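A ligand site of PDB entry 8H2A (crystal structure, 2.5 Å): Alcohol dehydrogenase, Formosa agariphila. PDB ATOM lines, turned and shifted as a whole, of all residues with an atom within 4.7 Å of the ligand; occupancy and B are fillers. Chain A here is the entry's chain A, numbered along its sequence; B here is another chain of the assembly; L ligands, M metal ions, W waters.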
ATOM      1  N   CYS A  41      18.787   6.476  11.082  1.00  0.00           N
ATOM      2  CA  CYS A  41      19.983   7.306  11.192  1.00  0.00           C
ATOM      3  C   CYS A  41      19.868   8.263  12.386  1.00  0.00           C
ATOM      4  O   CYS A  41      18.761   8.615  12.816  1.00  0.00           O
ATOM      5  CB  CYS A  41      20.183   8.108   9.899  1.00  0.00           C
ATOM      6  SG  CYS A  41      21.284   9.538  10.074  1.00  0.00           S
ATOM      7  N   HIS A  42      21.018   8.681  12.909  1.00  0.00           N
ATOM      8  CA  HIS A  42      21.030   9.689  13.980  1.00  0.00           C
ATOM      9  C   HIS A  42      20.283  10.979  13.583  1.00  0.00           C
ATOM     10  O   HIS A  42      19.728  11.663  14.453  1.00  0.00           O
ATOM     11  CB  HIS A  42      22.469  10.011  14.400  1.00  0.00           C
ATOM     12  CG  HIS A  42      22.578  10.900  15.612  1.00  0.00           C
ATOM     13  ND1 HIS A  42      22.347  12.257  15.558  1.00  0.00           N
ATOM     14  CD2 HIS A  42      22.905  10.613  16.890  1.00  0.00           C
ATOM     15  CE1 HIS A  42      22.522  12.771  16.764  1.00  0.00           C
ATOM     16  NE2 HIS A  42      22.859  11.798  17.591  1.00  0.00           N
ATOM     17  N   THR A  43      20.260  11.329  12.300  1.00  0.00           N
ATOM     18  CA  THR A  43      19.503  12.503  11.865  1.00  0.00           C
ATOM     19  C   THR A  43      17.986  12.303  12.005  1.00  0.00           C
ATOM     20  O   THR A  43      17.253  13.292  12.117  1.00  0.00           O
ATOM     21  CB  THR A  43      19.842  12.835  10.418  1.00  0.00           C
ATOM     22  OG1 THR A  43      21.265  12.897  10.277  1.00  0.00           O
ATOM     23  CG2 THR A  43      19.229  14.171  10.020  1.00  0.00           C
ATOM     24  N   ASP A  46      17.063  13.602  15.399  1.00  0.00           N
ATOM     25  CA  ASP A  46      17.095  15.054  15.292  1.00  0.00           C
ATOM     26  C   ASP A  46      15.823  15.594  14.625  1.00  0.00           C
ATOM     27  O   ASP A  46      15.447  16.757  14.859  1.00  0.00           O
ATOM     28  CB  ASP A  46      18.337  15.473  14.492  1.00  0.00           C
ATOM     29  CG  ASP A  46      19.639  15.261  15.264  1.00  0.00           C
ATOM     30  OD1 ASP A  46      19.716  15.739  16.415  1.00  0.00           O
ATOM     31  OD2 ASP A  46      20.601  14.642  14.730  1.00  0.00           O
ATOM     32  N   TRP A  84      18.223  10.418  -1.224  1.00  0.00           N
ATOM     33  CA  TRP A  84      17.709  11.756  -0.938  1.00  0.00           C
ATOM     34  C   TRP A  84      18.533  12.841  -1.615  1.00  0.00           C
ATOM     35  O   TRP A  84      18.475  14.002  -1.209  1.00  0.00           O
ATOM     36  CB  TRP A  84      17.597  12.048   0.564  1.00  0.00           C
ATOM     37  CG  TRP A  84      18.798  11.736   1.415  1.00  0.00           C
ATOM     38  CD1 TRP A  84      19.107  10.531   2.003  1.00  0.00           C
ATOM     39  CD2 TRP A  84      19.843  12.642   1.812  1.00  0.00           C
ATOM     40  NE1 TRP A  84      20.282  10.630   2.713  1.00  0.00           N
ATOM     41  CE2 TRP A  84      20.752  11.908   2.611  1.00  0.00           C
ATOM     42  CE3 TRP A  84      20.096  13.987   1.562  1.00  0.00           C
ATOM     43  CZ2 TRP A  84      21.904  12.492   3.159  1.00  0.00           C
ATOM     44  CZ3 TRP A  84      21.244  14.558   2.100  1.00  0.00           C
ATOM     45  CH2 TRP A  84      22.137  13.816   2.886  1.00  0.00           C
ATOM     46  N   CYS A 169      21.778   6.131   3.495  1.00  0.00           N
ATOM     47  CA  CYS A 169      22.431   7.229   4.198  1.00  0.00           C
ATOM     48  C   CYS A 169      23.739   6.767   4.838  1.00  0.00           C
ATOM     49  O   CYS A 169      24.823   7.119   4.350  1.00  0.00           O
ATOM     50  CB  CYS A 169      21.481   7.852   5.241  1.00  0.00           C
ATOM     51  SG  CYS A 169      22.074   9.397   6.081  1.00  0.00           S
ATOM     52  N   THR A 173      27.326   7.982   3.228  1.00  0.00           N
ATOM     53  CA  THR A 173      28.110   9.086   3.760  1.00  0.00           C
ATOM     54  C   THR A 173      29.436   8.589   4.313  1.00  0.00           C
ATOM     55  O   THR A 173      30.483   9.185   4.023  1.00  0.00           O
ATOM     56  CB  THR A 173      27.363   9.862   4.840  1.00  0.00           C
ATOM     57  OG1 THR A 173      27.506   9.155   6.073  1.00  0.00           O
ATOM     58  CG2 THR A 173      25.882  10.020   4.487  1.00  0.00           C
ATOM     59  N   GLY A 194      34.018   8.133  16.366  1.00  0.00           N
ATOM     60  CA  GLY A 194      32.608   7.819  16.335  1.00  0.00           C
ATOM     61  C   GLY A 194      32.289   6.694  15.381  1.00  0.00           C
ATOM     62  O   GLY A 194      31.944   6.932  14.234  1.00  0.00           O
ATOM     63  N   THR A 195      32.402   5.448  15.849  1.00  0.00           N
ATOM     64  CA  THR A 195      32.151   4.277  15.019  1.00  0.00           C
ATOM     65  C   THR A 195      30.698   3.823  15.179  1.00  0.00           C
ATOM     66  O   THR A 195      30.402   2.775  15.746  1.00  0.00           O
ATOM     67  CB  THR A 195      33.133   3.169  15.377  1.00  0.00           C
ATOM     68  OG1 THR A 195      32.757   2.560  16.625  1.00  0.00           O
ATOM     69  CG2 THR A 195      34.520   3.738  15.557  1.00  0.00           C
ATOM     70  N   GLY A 196      29.785   4.650  14.660  1.00  0.00           N
ATOM     71  CA  GLY A 196      28.361   4.354  14.747  1.00  0.00           C
ATOM     72  C   GLY A 196      27.718   3.992  13.432  1.00  0.00           C
ATOM     73  O   GLY A 196      28.277   3.220  12.646  1.00  0.00           O
ATOM     74  N   GLY A 197      26.543   4.558  13.154  1.00  0.00           N
ATOM     75  CA  GLY A 197      25.888   4.283  11.884  1.00  0.00           C
ATOM     76  C   GLY A 197      26.709   4.736  10.692  1.00  0.00           C
ATOM     77  O   GLY A 197      26.776   4.038   9.663  1.00  0.00           O
ATOM     78  N   VAL A 198      27.367   5.887  10.817  1.00  0.00           N
ATOM     79  CA  VAL A 198      28.222   6.377   9.740  1.00  0.00           C
ATOM     80  C   VAL A 198      29.655   5.908   9.914  1.00  0.00           C
ATOM     81  O   VAL A 198      30.278   5.398   8.967  1.00  0.00           O
ATOM     82  CB  VAL A 198      28.168   7.915   9.657  1.00  0.00           C
ATOM     83  CG1 VAL A 198      29.131   8.393   8.557  1.00  0.00           C
ATOM     84  CG2 VAL A 198      26.763   8.383   9.366  1.00  0.00           C
ATOM     85  N   GLY A 199      30.175   6.109  11.124  1.00  0.00           N
ATOM     86  CA  GLY A 199      31.578   5.833  11.388  1.00  0.00           C
ATOM     87  C   GLY A 199      31.987   4.415  11.077  1.00  0.00           C
ATOM     88  O   GLY A 199      33.106   4.173  10.605  1.00  0.00           O
ATOM     89  N   ILE A 217      37.855   5.121  17.478  1.00  0.00           N
ATOM     90  CA  ILE A 217      37.764   5.822  18.746  1.00  0.00           C
ATOM     91  C   ILE A 217      36.288   6.059  19.029  1.00  0.00           C
ATOM     92  O   ILE A 217      35.593   6.663  18.208  1.00  0.00           O
ATOM     93  CB  ILE A 217      38.535   7.160  18.740  1.00  0.00           C
ATOM     94  CG1 ILE A 217      39.965   6.934  18.206  1.00  0.00           C
ATOM     95  CG2 ILE A 217      38.506   7.802  20.131  1.00  0.00           C
ATOM     96  CD1 ILE A 217      40.796   8.183  18.051  1.00  0.00           C
ATOM     97  N   ASP A 218      35.816   5.552  20.178  1.00  0.00           N
ATOM     98  CA  ASP A 218      34.442   5.706  20.622  1.00  0.00           C
ATOM     99  C   ASP A 218      34.412   5.675  22.149  1.00  0.00           C
ATOM    100  O   ASP A 218      35.341   5.173  22.790  1.00  0.00           O
ATOM    101  CB  ASP A 218      33.518   4.596  20.079  1.00  0.00           C
ATOM    102  CG  ASP A 218      32.079   5.043  19.935  1.00  0.00           C
ATOM    103  OD1 ASP A 218      31.372   5.166  20.953  1.00  0.00           O
ATOM    104  OD2 ASP A 218      31.635   5.252  18.793  1.00  0.00           O
ATOM    105  N   ILE A 219      33.320   6.199  22.716  1.00  0.00           N
ATOM    106  CA  ILE A 219      33.093   6.120  24.152  1.00  0.00           C
ATOM    107  C   ILE A 219      32.446   4.812  24.581  1.00  0.00           C
ATOM    108  O   ILE A 219      32.440   4.507  25.777  1.00  0.00           O
ATOM    109  CB  ILE A 219      32.205   7.267  24.639  1.00  0.00           C
ATOM    110  CG1 ILE A 219      30.886   7.234  23.883  1.00  0.00           C
ATOM    111  CG2 ILE A 219      32.900   8.609  24.459  1.00  0.00           C
ATOM    112  CD1 ILE A 219      29.912   8.272  24.299  1.00  0.00           C
ATOM    113  N   ASN A 220      31.884   4.034  23.658  1.00  0.00           N
ATOM    114  CA  ASN A 220      31.202   2.789  23.989  1.00  0.00           C
ATOM    115  C   ASN A 220      31.975   1.590  23.465  1.00  0.00           C
ATOM    116  O   ASN A 220      32.343   1.538  22.289  1.00  0.00           O
ATOM    117  CB  ASN A 220      29.771   2.772  23.427  1.00  0.00           C
ATOM    118  CG  ASN A 220      29.046   1.462  23.723  1.00  0.00           C
ATOM    119  OD1 ASN A 220      29.168   0.895  24.816  1.00  0.00           O
ATOM    120  ND2 ASN A 220      28.284   0.977  22.757  1.00  0.00           N
ATOM    121  N   ARG A 223      30.255  -0.551  20.268  1.00  0.00           N
ATOM    122  CA  ARG A 223      30.672   0.236  19.111  1.00  0.00           C
ATOM    123  C   ARG A 223      32.079  -0.112  18.648  1.00  0.00           C
ATOM    124  O   ARG A 223      32.279  -0.464  17.476  1.00  0.00           O
ATOM    125  CB  ARG A 223      30.512   1.729  19.448  1.00  0.00           C
ATOM    126  CG  ARG A 223      29.011   1.995  19.595  1.00  0.00           C
ATOM    127  CD  ARG A 223      28.288   2.017  18.202  1.00  0.00           C
ATOM    128  NE  ARG A 223      26.826   1.843  18.259  1.00  0.00           N
ATOM    129  CZ  ARG A 223      25.863   2.737  18.500  1.00  0.00           C
ATOM    130  NH1 ARG A 223      26.124   4.002  18.821  1.00  0.00           N
ATOM    131  NH2 ARG A 223      24.609   2.316  18.477  1.00  0.00           N
ATOM    132  N   ALA A 238      37.555   6.239  24.210  1.00  0.00           N
ATOM    133  CA  ALA A 238      37.572   7.604  24.701  1.00  0.00           C
ATOM    134  C   ALA A 238      36.684   7.770  25.932  1.00  0.00           C
ATOM    135  O   ALA A 238      35.644   7.107  26.073  1.00  0.00           O
ATOM    136  CB  ALA A 238      37.104   8.537  23.601  1.00  0.00           C
ATOM    137  N   LYS A 240      34.232  10.324  27.752  1.00  0.00           N
ATOM    138  CA  LYS A 240      33.419  11.423  27.239  1.00  0.00           C
ATOM    139  C   LYS A 240      33.804  12.751  27.882  1.00  0.00           C
ATOM    140  O   LYS A 240      33.682  13.800  27.238  1.00  0.00           O
ATOM    141  CB  LYS A 240      31.933  11.133  27.438  1.00  0.00           C
ATOM    142  CG  LYS A 240      31.026  12.241  26.870  1.00  0.00           C
ATOM    143  CD  LYS A 240      29.525  11.928  27.007  1.00  0.00           C
ATOM    144  CE  LYS A 240      28.985  11.226  25.770  1.00  0.00           C
ATOM    145  NZ  LYS A 240      28.952  12.088  24.539  1.00  0.00           N
ATOM    146  N   LEU A 245      38.771  15.472  22.740  1.00  0.00           N
ATOM    147  CA  LEU A 245      39.501  14.221  22.526  1.00  0.00           C
ATOM    148  C   LEU A 245      41.003  14.466  22.361  1.00  0.00           C
ATOM    149  O   LEU A 245      41.713  13.715  21.690  1.00  0.00           O
ATOM    150  CB  LEU A 245      38.951  13.462  21.310  1.00  0.00           C
ATOM    151  CG  LEU A 245      37.523  12.938  21.425  1.00  0.00           C
ATOM    152  CD1 LEU A 245      36.932  12.786  20.030  1.00  0.00           C
ATOM    153  CD2 LEU A 245      37.477  11.588  22.165  1.00  0.00           C
ATOM    154  N   CYS A 267      32.452  11.949  13.246  1.00  0.00           N
ATOM    155  CA  CYS A 267      31.102  11.407  13.182  1.00  0.00           C
ATOM    156  C   CYS A 267      30.685  10.970  14.570  1.00  0.00           C
ATOM    157  O   CYS A 267      30.268   9.836  14.787  1.00  0.00           O
ATOM    158  CB  CYS A 267      31.033  10.330  12.105  1.00  0.00           C
ATOM    159  SG  CYS A 267      32.267   9.038  12.185  1.00  0.00           S
ATOM    160  N   THR A 268      30.816  11.896  15.521  1.00  0.00           N
ATOM    161  CA  THR A 268      30.461  11.694  16.920  1.00  0.00           C
ATOM    162  C   THR A 268      29.079  12.226  17.269  1.00  0.00           C
ATOM    163  O   THR A 268      28.540  11.856  18.311  1.00  0.00           O
ATOM    164  CB  THR A 268      31.480  12.381  17.849  1.00  0.00           C
ATOM    165  OG1 THR A 268      31.350  13.807  17.727  1.00  0.00           O
ATOM    166  CG2 THR A 268      32.892  11.990  17.479  1.00  0.00           C
ATOM    167  N   ALA A 269      28.491  13.093  16.436  1.00  0.00           N
ATOM    168  CA  ALA A 269      27.253  13.821  16.720  1.00  0.00           C
ATOM    169  C   ALA A 269      27.394  14.774  17.894  1.00  0.00           C
ATOM    170  O   ALA A 269      26.389  15.266  18.426  1.00  0.00           O
ATOM    171  CB  ALA A 269      26.068  12.869  16.980  1.00  0.00           C
ATOM    172  N   ILE A 270      28.620  15.082  18.311  1.00  0.00           N
ATOM    173  CA  ILE A 270      28.858  16.023  19.390  1.00  0.00           C
ATOM    174  C   ILE A 270      29.359  17.325  18.765  1.00  0.00           C
ATOM    175  O   ILE A 270      30.466  17.342  18.211  1.00  0.00           O
ATOM    176  CB  ILE A 270      29.855  15.468  20.409  1.00  0.00           C
ATOM    177  CG1 ILE A 270      29.266  14.208  21.059  1.00  0.00           C
ATOM    178  CG2 ILE A 270      30.174  16.538  21.456  1.00  0.00           C
ATOM    179  CD1 ILE A 270      27.929  14.468  21.759  1.00  0.00           C
ATOM    180  N   LEU A 273      33.042  18.476  19.433  1.00  0.00           N
ATOM    181  CA  LEU A 273      34.143  17.766  18.822  1.00  0.00           C
ATOM    182  C   LEU A 273      34.332  18.151  17.339  1.00  0.00           C
ATOM    183  O   LEU A 273      34.992  17.415  16.589  1.00  0.00           O
ATOM    184  CB  LEU A 273      33.917  16.260  18.991  1.00  0.00           C
ATOM    185  CG  LEU A 273      33.861  15.830  20.457  1.00  0.00           C
ATOM    186  CD1 LEU A 273      33.758  14.321  20.615  1.00  0.00           C
ATOM    187  CD2 LEU A 273      35.063  16.336  21.198  1.00  0.00           C
ATOM    188  N   VAL A 290      32.065  14.607   9.180  1.00  0.00           N
ATOM    189  CA  VAL A 290      30.843  14.084   8.558  1.00  0.00           C
ATOM    190  C   VAL A 290      29.566  14.494   9.303  1.00  0.00           C
ATOM    191  O   VAL A 290      28.480  14.487   8.695  1.00  0.00           O
ATOM    192  CB  VAL A 290      30.952  12.551   8.467  1.00  0.00           C
ATOM    193  CG1 VAL A 290      29.807  11.941   7.638  1.00  0.00           C
ATOM    194  CG2 VAL A 290      32.314  12.162   7.898  1.00  0.00           C
ATOM    195  N   SER A 291      29.665  14.884  10.572  1.00  0.00           N
ATOM    196  CA  SER A 291      28.453  15.001  11.378  1.00  0.00           C
ATOM    197  C   SER A 291      27.545  16.100  10.840  1.00  0.00           C
ATOM    198  O   SER A 291      26.363  15.870  10.579  1.00  0.00           O
ATOM    199  CB  SER A 291      28.808  15.267  12.843  1.00  0.00           C
ATOM    200  OG  SER A 291      29.180  14.051  13.482  1.00  0.00           O
ATOM    201  N   PRO A 313      31.679  17.482   4.458  1.00  0.00           N
ATOM    202  CA  PRO A 313      30.942  17.040   3.272  1.00  0.00           C
ATOM    203  C   PRO A 313      29.553  16.524   3.626  1.00  0.00           C
ATOM    204  O   PRO A 313      29.254  16.199   4.776  1.00  0.00           O
ATOM    205  CB  PRO A 313      31.827  15.935   2.682  1.00  0.00           C
ATOM    206  CG  PRO A 313      32.563  15.382   3.832  1.00  0.00           C
ATOM    207  CD  PRO A 313      32.724  16.523   4.841  1.00  0.00           C
ATOM    208  N   LEU A 314      28.694  16.460   2.600  1.00  0.00           N
ATOM    209  CA  LEU A 314      27.302  16.006   2.719  1.00  0.00           C
ATOM    210  C   LEU A 314      27.111  14.750   1.882  1.00  0.00           C
ATOM    211  O   LEU A 314      27.429  14.741   0.697  1.00  0.00           O
ATOM    212  CB  LEU A 314      26.331  17.098   2.262  1.00  0.00           C
ATOM    213  CG  LEU A 314      24.831  16.725   2.341  1.00  0.00           C
ATOM    214  CD1 LEU A 314      24.273  16.770   3.791  1.00  0.00           C
ATOM    215  CD2 LEU A 314      23.940  17.549   1.380  1.00  0.00           C
ATOM    216  N   TYR A 315      26.629  13.676   2.522  1.00  0.00           N
ATOM    217  CA  TYR A 315      26.123  12.496   1.814  1.00  0.00           C
ATOM    218  C   TYR A 315      27.225  11.791   1.032  1.00  0.00           C
ATOM    219  O   TYR A 315      26.985  11.169  -0.008  1.00  0.00           O
ATOM    220  CB  TYR A 315      24.921  12.892   0.940  1.00  0.00           C
ATOM    221  CG  TYR A 315      23.965  11.792   0.513  1.00  0.00           C
ATOM    222  CD1 TYR A 315      23.838  10.627   1.253  1.00  0.00           C
ATOM    223  CD2 TYR A 315      23.081  11.999  -0.547  1.00  0.00           C
ATOM    224  CE1 TYR A 315      22.937   9.633   0.891  1.00  0.00           C
ATOM    225  CE2 TYR A 315      22.173  11.023  -0.911  1.00  0.00           C
ATOM    226  CZ  TYR A 315      22.102   9.835  -0.191  1.00  0.00           C
ATOM    227  OH  TYR A 315      21.188   8.869  -0.546  1.00  0.00           O
ATOM    228  N   MET A 358      19.839   2.605  19.096  1.00  0.00           N
ATOM    229  CA  MET A 358      20.873   3.348  18.373  1.00  0.00           C
ATOM    230  C   MET A 358      21.667   4.247  19.309  1.00  0.00           C
ATOM    231  O   MET A 358      22.904   4.312  19.230  1.00  0.00           O
ATOM    232  CB  MET A 358      20.244   4.155  17.242  1.00  0.00           C
ATOM    233  CG  MET A 358      21.264   4.982  16.443  1.00  0.00           C
ATOM    234  SD  MET A 358      20.516   6.443  15.685  1.00  0.00           S
ATOM    235  CE  MET A 358      19.139   5.752  14.811  1.00  0.00           C
ATOM    236  N   LEU A 359      20.966   4.957  20.196  1.00  0.00           N
ATOM    237  CA  LEU A 359      21.597   5.914  21.093  1.00  0.00           C
ATOM    238  C   LEU A 359      22.256   5.246  22.286  1.00  0.00           C
ATOM    239  O   LEU A 359      23.263   5.744  22.803  1.00  0.00           O
ATOM    240  CB  LEU A 359      20.561   6.922  21.572  1.00  0.00           C
ATOM    241  CG  LEU A 359      19.851   7.558  20.372  1.00  0.00           C
ATOM    242  CD1 LEU A 359      18.719   8.498  20.807  1.00  0.00           C
ATOM    243  CD2 LEU A 359      20.903   8.260  19.502  1.00  0.00           C
ATOM    244  N   LYS A 365      23.384  -0.688  13.221  1.00  0.00           N
ATOM    245  CA  LYS A 365      22.332   0.068  12.581  1.00  0.00           C
ATOM    246  C   LYS A 365      21.045  -0.693  12.899  1.00  0.00           C
ATOM    247  O   LYS A 365      21.080  -1.880  13.190  1.00  0.00           O
ATOM    248  CB  LYS A 365      22.597   0.188  11.069  1.00  0.00           C
ATOM    249  CG  LYS A 365      21.530   0.864  10.237  1.00  0.00           C
ATOM    250  CD  LYS A 365      21.495   2.350  10.422  1.00  0.00           C
ATOM    251  CE  LYS A 365      22.614   3.051   9.694  1.00  0.00           C
ATOM    252  NZ  LYS A 365      22.347   4.520   9.701  1.00  0.00           N
ATOM    253  N   TRP B 306      29.222  22.243   3.899  1.00  0.00           N
ATOM    254  CA  TRP B 306      28.804  21.676   2.637  1.00  0.00           C
ATOM    255  C   TRP B 306      29.933  21.788   1.637  1.00  0.00           C
ATOM    256  O   TRP B 306      30.011  22.694   0.797  1.00  0.00           O
ATOM    257  CB  TRP B 306      27.471  22.328   2.351  1.00  0.00           C
ATOM    258  CG  TRP B 306      26.276  21.641   3.107  1.00  0.00           C
ATOM    259  CD1 TRP B 306      25.114  21.289   2.539  1.00  0.00           C
ATOM    260  CD2 TRP B 306      26.329  20.817   4.320  1.00  0.00           C
ATOM    261  NE1 TRP B 306      24.308  20.626   3.417  1.00  0.00           N
ATOM    262  CE2 TRP B 306      25.057  20.267   4.501  1.00  0.00           C
ATOM    263  CE3 TRP B 306      27.293  20.573   5.313  1.00  0.00           C
ATOM    264  CZ2 TRP B 306      24.709  19.483   5.618  1.00  0.00           C
ATOM    265  CZ3 TRP B 306      26.937  19.807   6.438  1.00  0.00           C
ATOM    266  CH2 TRP B 306      25.656  19.270   6.567  1.00  0.00           C
HETATM  267  P1  LIG L   1      25.208   7.285  16.007  1.00  0.00           P
HETATM  268  O1  LIG L   1      24.567   7.747  17.307  1.00  0.00           O
HETATM  269  O2  LIG L   1      24.607   5.947  15.522  1.00  0.00           O
HETATM  270  O3  LIG L   1      26.867   7.060  16.248  1.00  0.00           O
HETATM  271  C1  LIG L   1      27.536   8.108  16.915  1.00  0.00           C
HETATM  272  C2  LIG L   1      28.821   7.511  17.516  1.00  0.00           C
HETATM  273  O4  LIG L   1      29.452   8.517  18.037  1.00  0.00           O
HETATM  274  C3  LIG L   1      28.488   6.544  18.703  1.00  0.00           C
HETATM  275  O5  LIG L   1      29.209   5.369  18.626  1.00  0.00           O
HETATM  276  C4  LIG L   1      28.894   7.384  19.913  1.00  0.00           C
HETATM  277  O6  LIG L   1      29.209   6.571  21.106  1.00  0.00           O
HETATM  278  C5  LIG L   1      29.977   8.001  19.466  1.00  0.00           C
HETATM  279  N1  LIG L   1      30.384   9.079  20.334  1.00  0.00           N
HETATM  280  C6  LIG L   1      29.644   9.987  20.964  1.00  0.00           C
HETATM  281  N2  LIG L   1      30.448  10.798  21.641  1.00  0.00           N
HETATM  282  C7  LIG L   1      31.686  10.395  21.447  1.00  0.00           C
HETATM  283  C8  LIG L   1      32.874  10.876  21.903  1.00  0.00           C
HETATM  284  N3  LIG L   1      33.145  11.939  22.760  1.00  0.00           N
HETATM  285  N4  LIG L   1      34.004  10.277  21.516  1.00  0.00           N
HETATM  286  C9  LIG L   1      33.975   9.200  20.698  1.00  0.00           C
HETATM  287  N5  LIG L   1      32.812   8.740  20.236  1.00  0.00           N
HETATM  288  C10 LIG L   1      31.658   9.340  20.629  1.00  0.00           C
HETATM  289  O7  LIG L   1      25.004   8.442  14.839  1.00  0.00           O
HETATM  290  P2  LIG L   1      25.331   8.245  13.165  1.00  0.00           P
HETATM  291  O8  LIG L   1      24.096   7.675  12.462  1.00  0.00           O
HETATM  292  O9  LIG L   1      26.572   7.325  12.909  1.00  0.00           O
HETATM  293  O10 LIG L   1      25.638   9.722  12.595  1.00  0.00           O
HETATM  294  C11 LIG L   1      26.638  10.462  13.265  1.00  0.00           C
HETATM  295  C12 LIG L   1      26.564  11.944  12.816  1.00  0.00           C
HETATM  296  O11 LIG L   1      26.675  12.042  11.513  1.00  0.00           O
HETATM  297  C13 LIG L   1      25.186  12.580  13.202  1.00  0.00           C
HETATM  298  O12 LIG L   1      25.493  13.854  13.632  1.00  0.00           O
HETATM  299  C14 LIG L   1      24.421  12.624  11.883  1.00  0.00           C
HETATM  300  O13 LIG L   1      23.362  13.662  11.891  1.00  0.00           O
HETATM  301  C15 LIG L   1      25.417  12.922  11.018  1.00  0.00           C
HETATM  302  N6  LIG L   1      25.155  12.562   9.642  1.00  0.00           N
HETATM  303  C16 LIG L   1      25.624  13.355   8.645  1.00  0.00           C
HETATM  304  C17 LIG L   1      25.420  13.019   7.256  1.00  0.00           C
HETATM  305  C18 LIG L   1      25.939  13.895   6.123  1.00  0.00           C
HETATM  306  O14 LIG L   1      25.465  13.810   5.007  1.00  0.00           O
HETATM  307  N7  LIG L   1      27.033  14.861   6.374  1.00  0.00           N
HETATM  308  C19 LIG L   1      24.767  11.909   6.979  1.00  0.00           C
HETATM  309  C20 LIG L   1      24.309  11.111   7.988  1.00  0.00           C
HETATM  310  C21 LIG L   1      24.524  11.451   9.368  1.00  0.00           C
HETATM  311 ZN    ZN M   1      21.173  10.449   7.927  1.00  0.00          ZN
HETATM  312  O   HOH W   1      35.069  13.560  24.822  1.00  0.00           O
HETATM  313  O   HOH W   2      21.672  12.287   7.537  1.00  0.00           O
HETATM  314  O   HOH W   3      26.425   6.085  22.808  1.00  0.00           O
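The backbone carbonyl oxygen (O) of Val 290 lies within hydrogen-bond range of a nitrogen (N7) of the ligand (2.8 Å). O5 of the ligand is in hydrogen-bond range of NH1 of Arg 223, at 3.4 Å. OD2 of Asp 218 lies within hydrogen-bond range of O5 of the ligand, 2.4 Å away. O of Pro 313 is in hydrogen-bond range of N7 of the ligand (3.0 Å). O9 of the ligand lies within hydrogen-bond range of N of Gly 197 (2.8 Å). The backbone NH (N) of Tyr 315 is in hydrogen-bond range of an oxygen (O14) of the ligand (2.7 Å). The backbone NH (N) of Val 198 lies within hydrogen-bond range of an oxygen (O9) of the ligand (2.7 Å). An oxygen (O13) of the ligand lies within hydrogen-bond range of the side-chain hydroxyl of Thr 43 (2.8 Å). The backbone NH (N) of His 42 sits at hydrogen-bond distance from an oxygen (O8) of the ligand (3.3 Å).
N of Ala 238 lies within hydrogen-bond range of O of Asp 218, at 2.8 Å. OG of Ser 291 is in hydrogen-bond range of N of Thr 268, at 3.4 Å. NH2 of Arg 223 sits at hydrogen-bond distance from O of Met 358, at 2.7 Å. The side-chain hydroxyl of Thr 268 sits at hydrogen-bond distance from the backbone NH of Ile 270 (3.1 Å). The backbone NH of Thr 43 sits close to the side-chain sulfur of Cys 41 (3.0 Å). N of Gly 199 sits close to SG of Cys 267, 3.8 Å away. The backbone NH (N) of Gly 194 is in hydrogen-bond range of the backbone carbonyl oxygen (O) of Ile 217, 2.8 Å away. The backbone NH (N) of Trp 84 is in hydrogen-bond range of the side-chain hydroxyl (OH) of Tyr 315 (3.4 Å).
An oxygen (O4) of the ligand lies close to the backbone carbonyl oxygen (O) of Thr 268 (3.5 Å). Merely in contact with the ligand: Cys 41 (3.8 Å), Trp 84 (3.9 Å), Cys 169 (3.4 Å), Thr 173 (3.3 Å), Gly 194 (3.7 Å), Gly 196 (3.4 Å), Ile 217 (3.9 Å), Ile 219 (3.3 Å), Lys 240 (3.5 Å), Leu 245 (3.8 Å), Cys 267 (3.6 Å), Ala 269 (3.5 Å), Ile 270 (3.7 Å), Leu 273 (3.3 Å), Ser 291 (3.1 Å), Leu 314 (3.4 Å) and Met 358 (3.6 Å). Hydrophobic or aromatic side chains within 4 Å of the ligand: His 42, Trp 84, Val 198, Ile 219, Leu 245, Ala 269, Ile 270, Leu 273, Leu 314 and Met 358. Within 4 Å of the ligand: Cys 41, His 42, Thr 43, Trp 84, Cys 169, Thr 173, Gly 194, Gly 196, Gly 197, Val 198, Ile 217, Asp 218, Ile 219, Arg 223, Lys 240, Leu 245, Cys 267, Thr 268, Ala 269, Ile 270, Leu 273, Val 290, Ser 291, Pro 313, Leu 314, Tyr 315 and Met 358. Along chain A the residues within 4 Å of the ligand span positions 41 to 358.
Water W1 bridges O of Lys 240 (2.8 Å) and N3 of the ligand (3.3 Å). Water W3 lies within hydrogen-bond range of O of Leu 359 (3.2 Å) and O6 of the ligand (3.3 Å).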
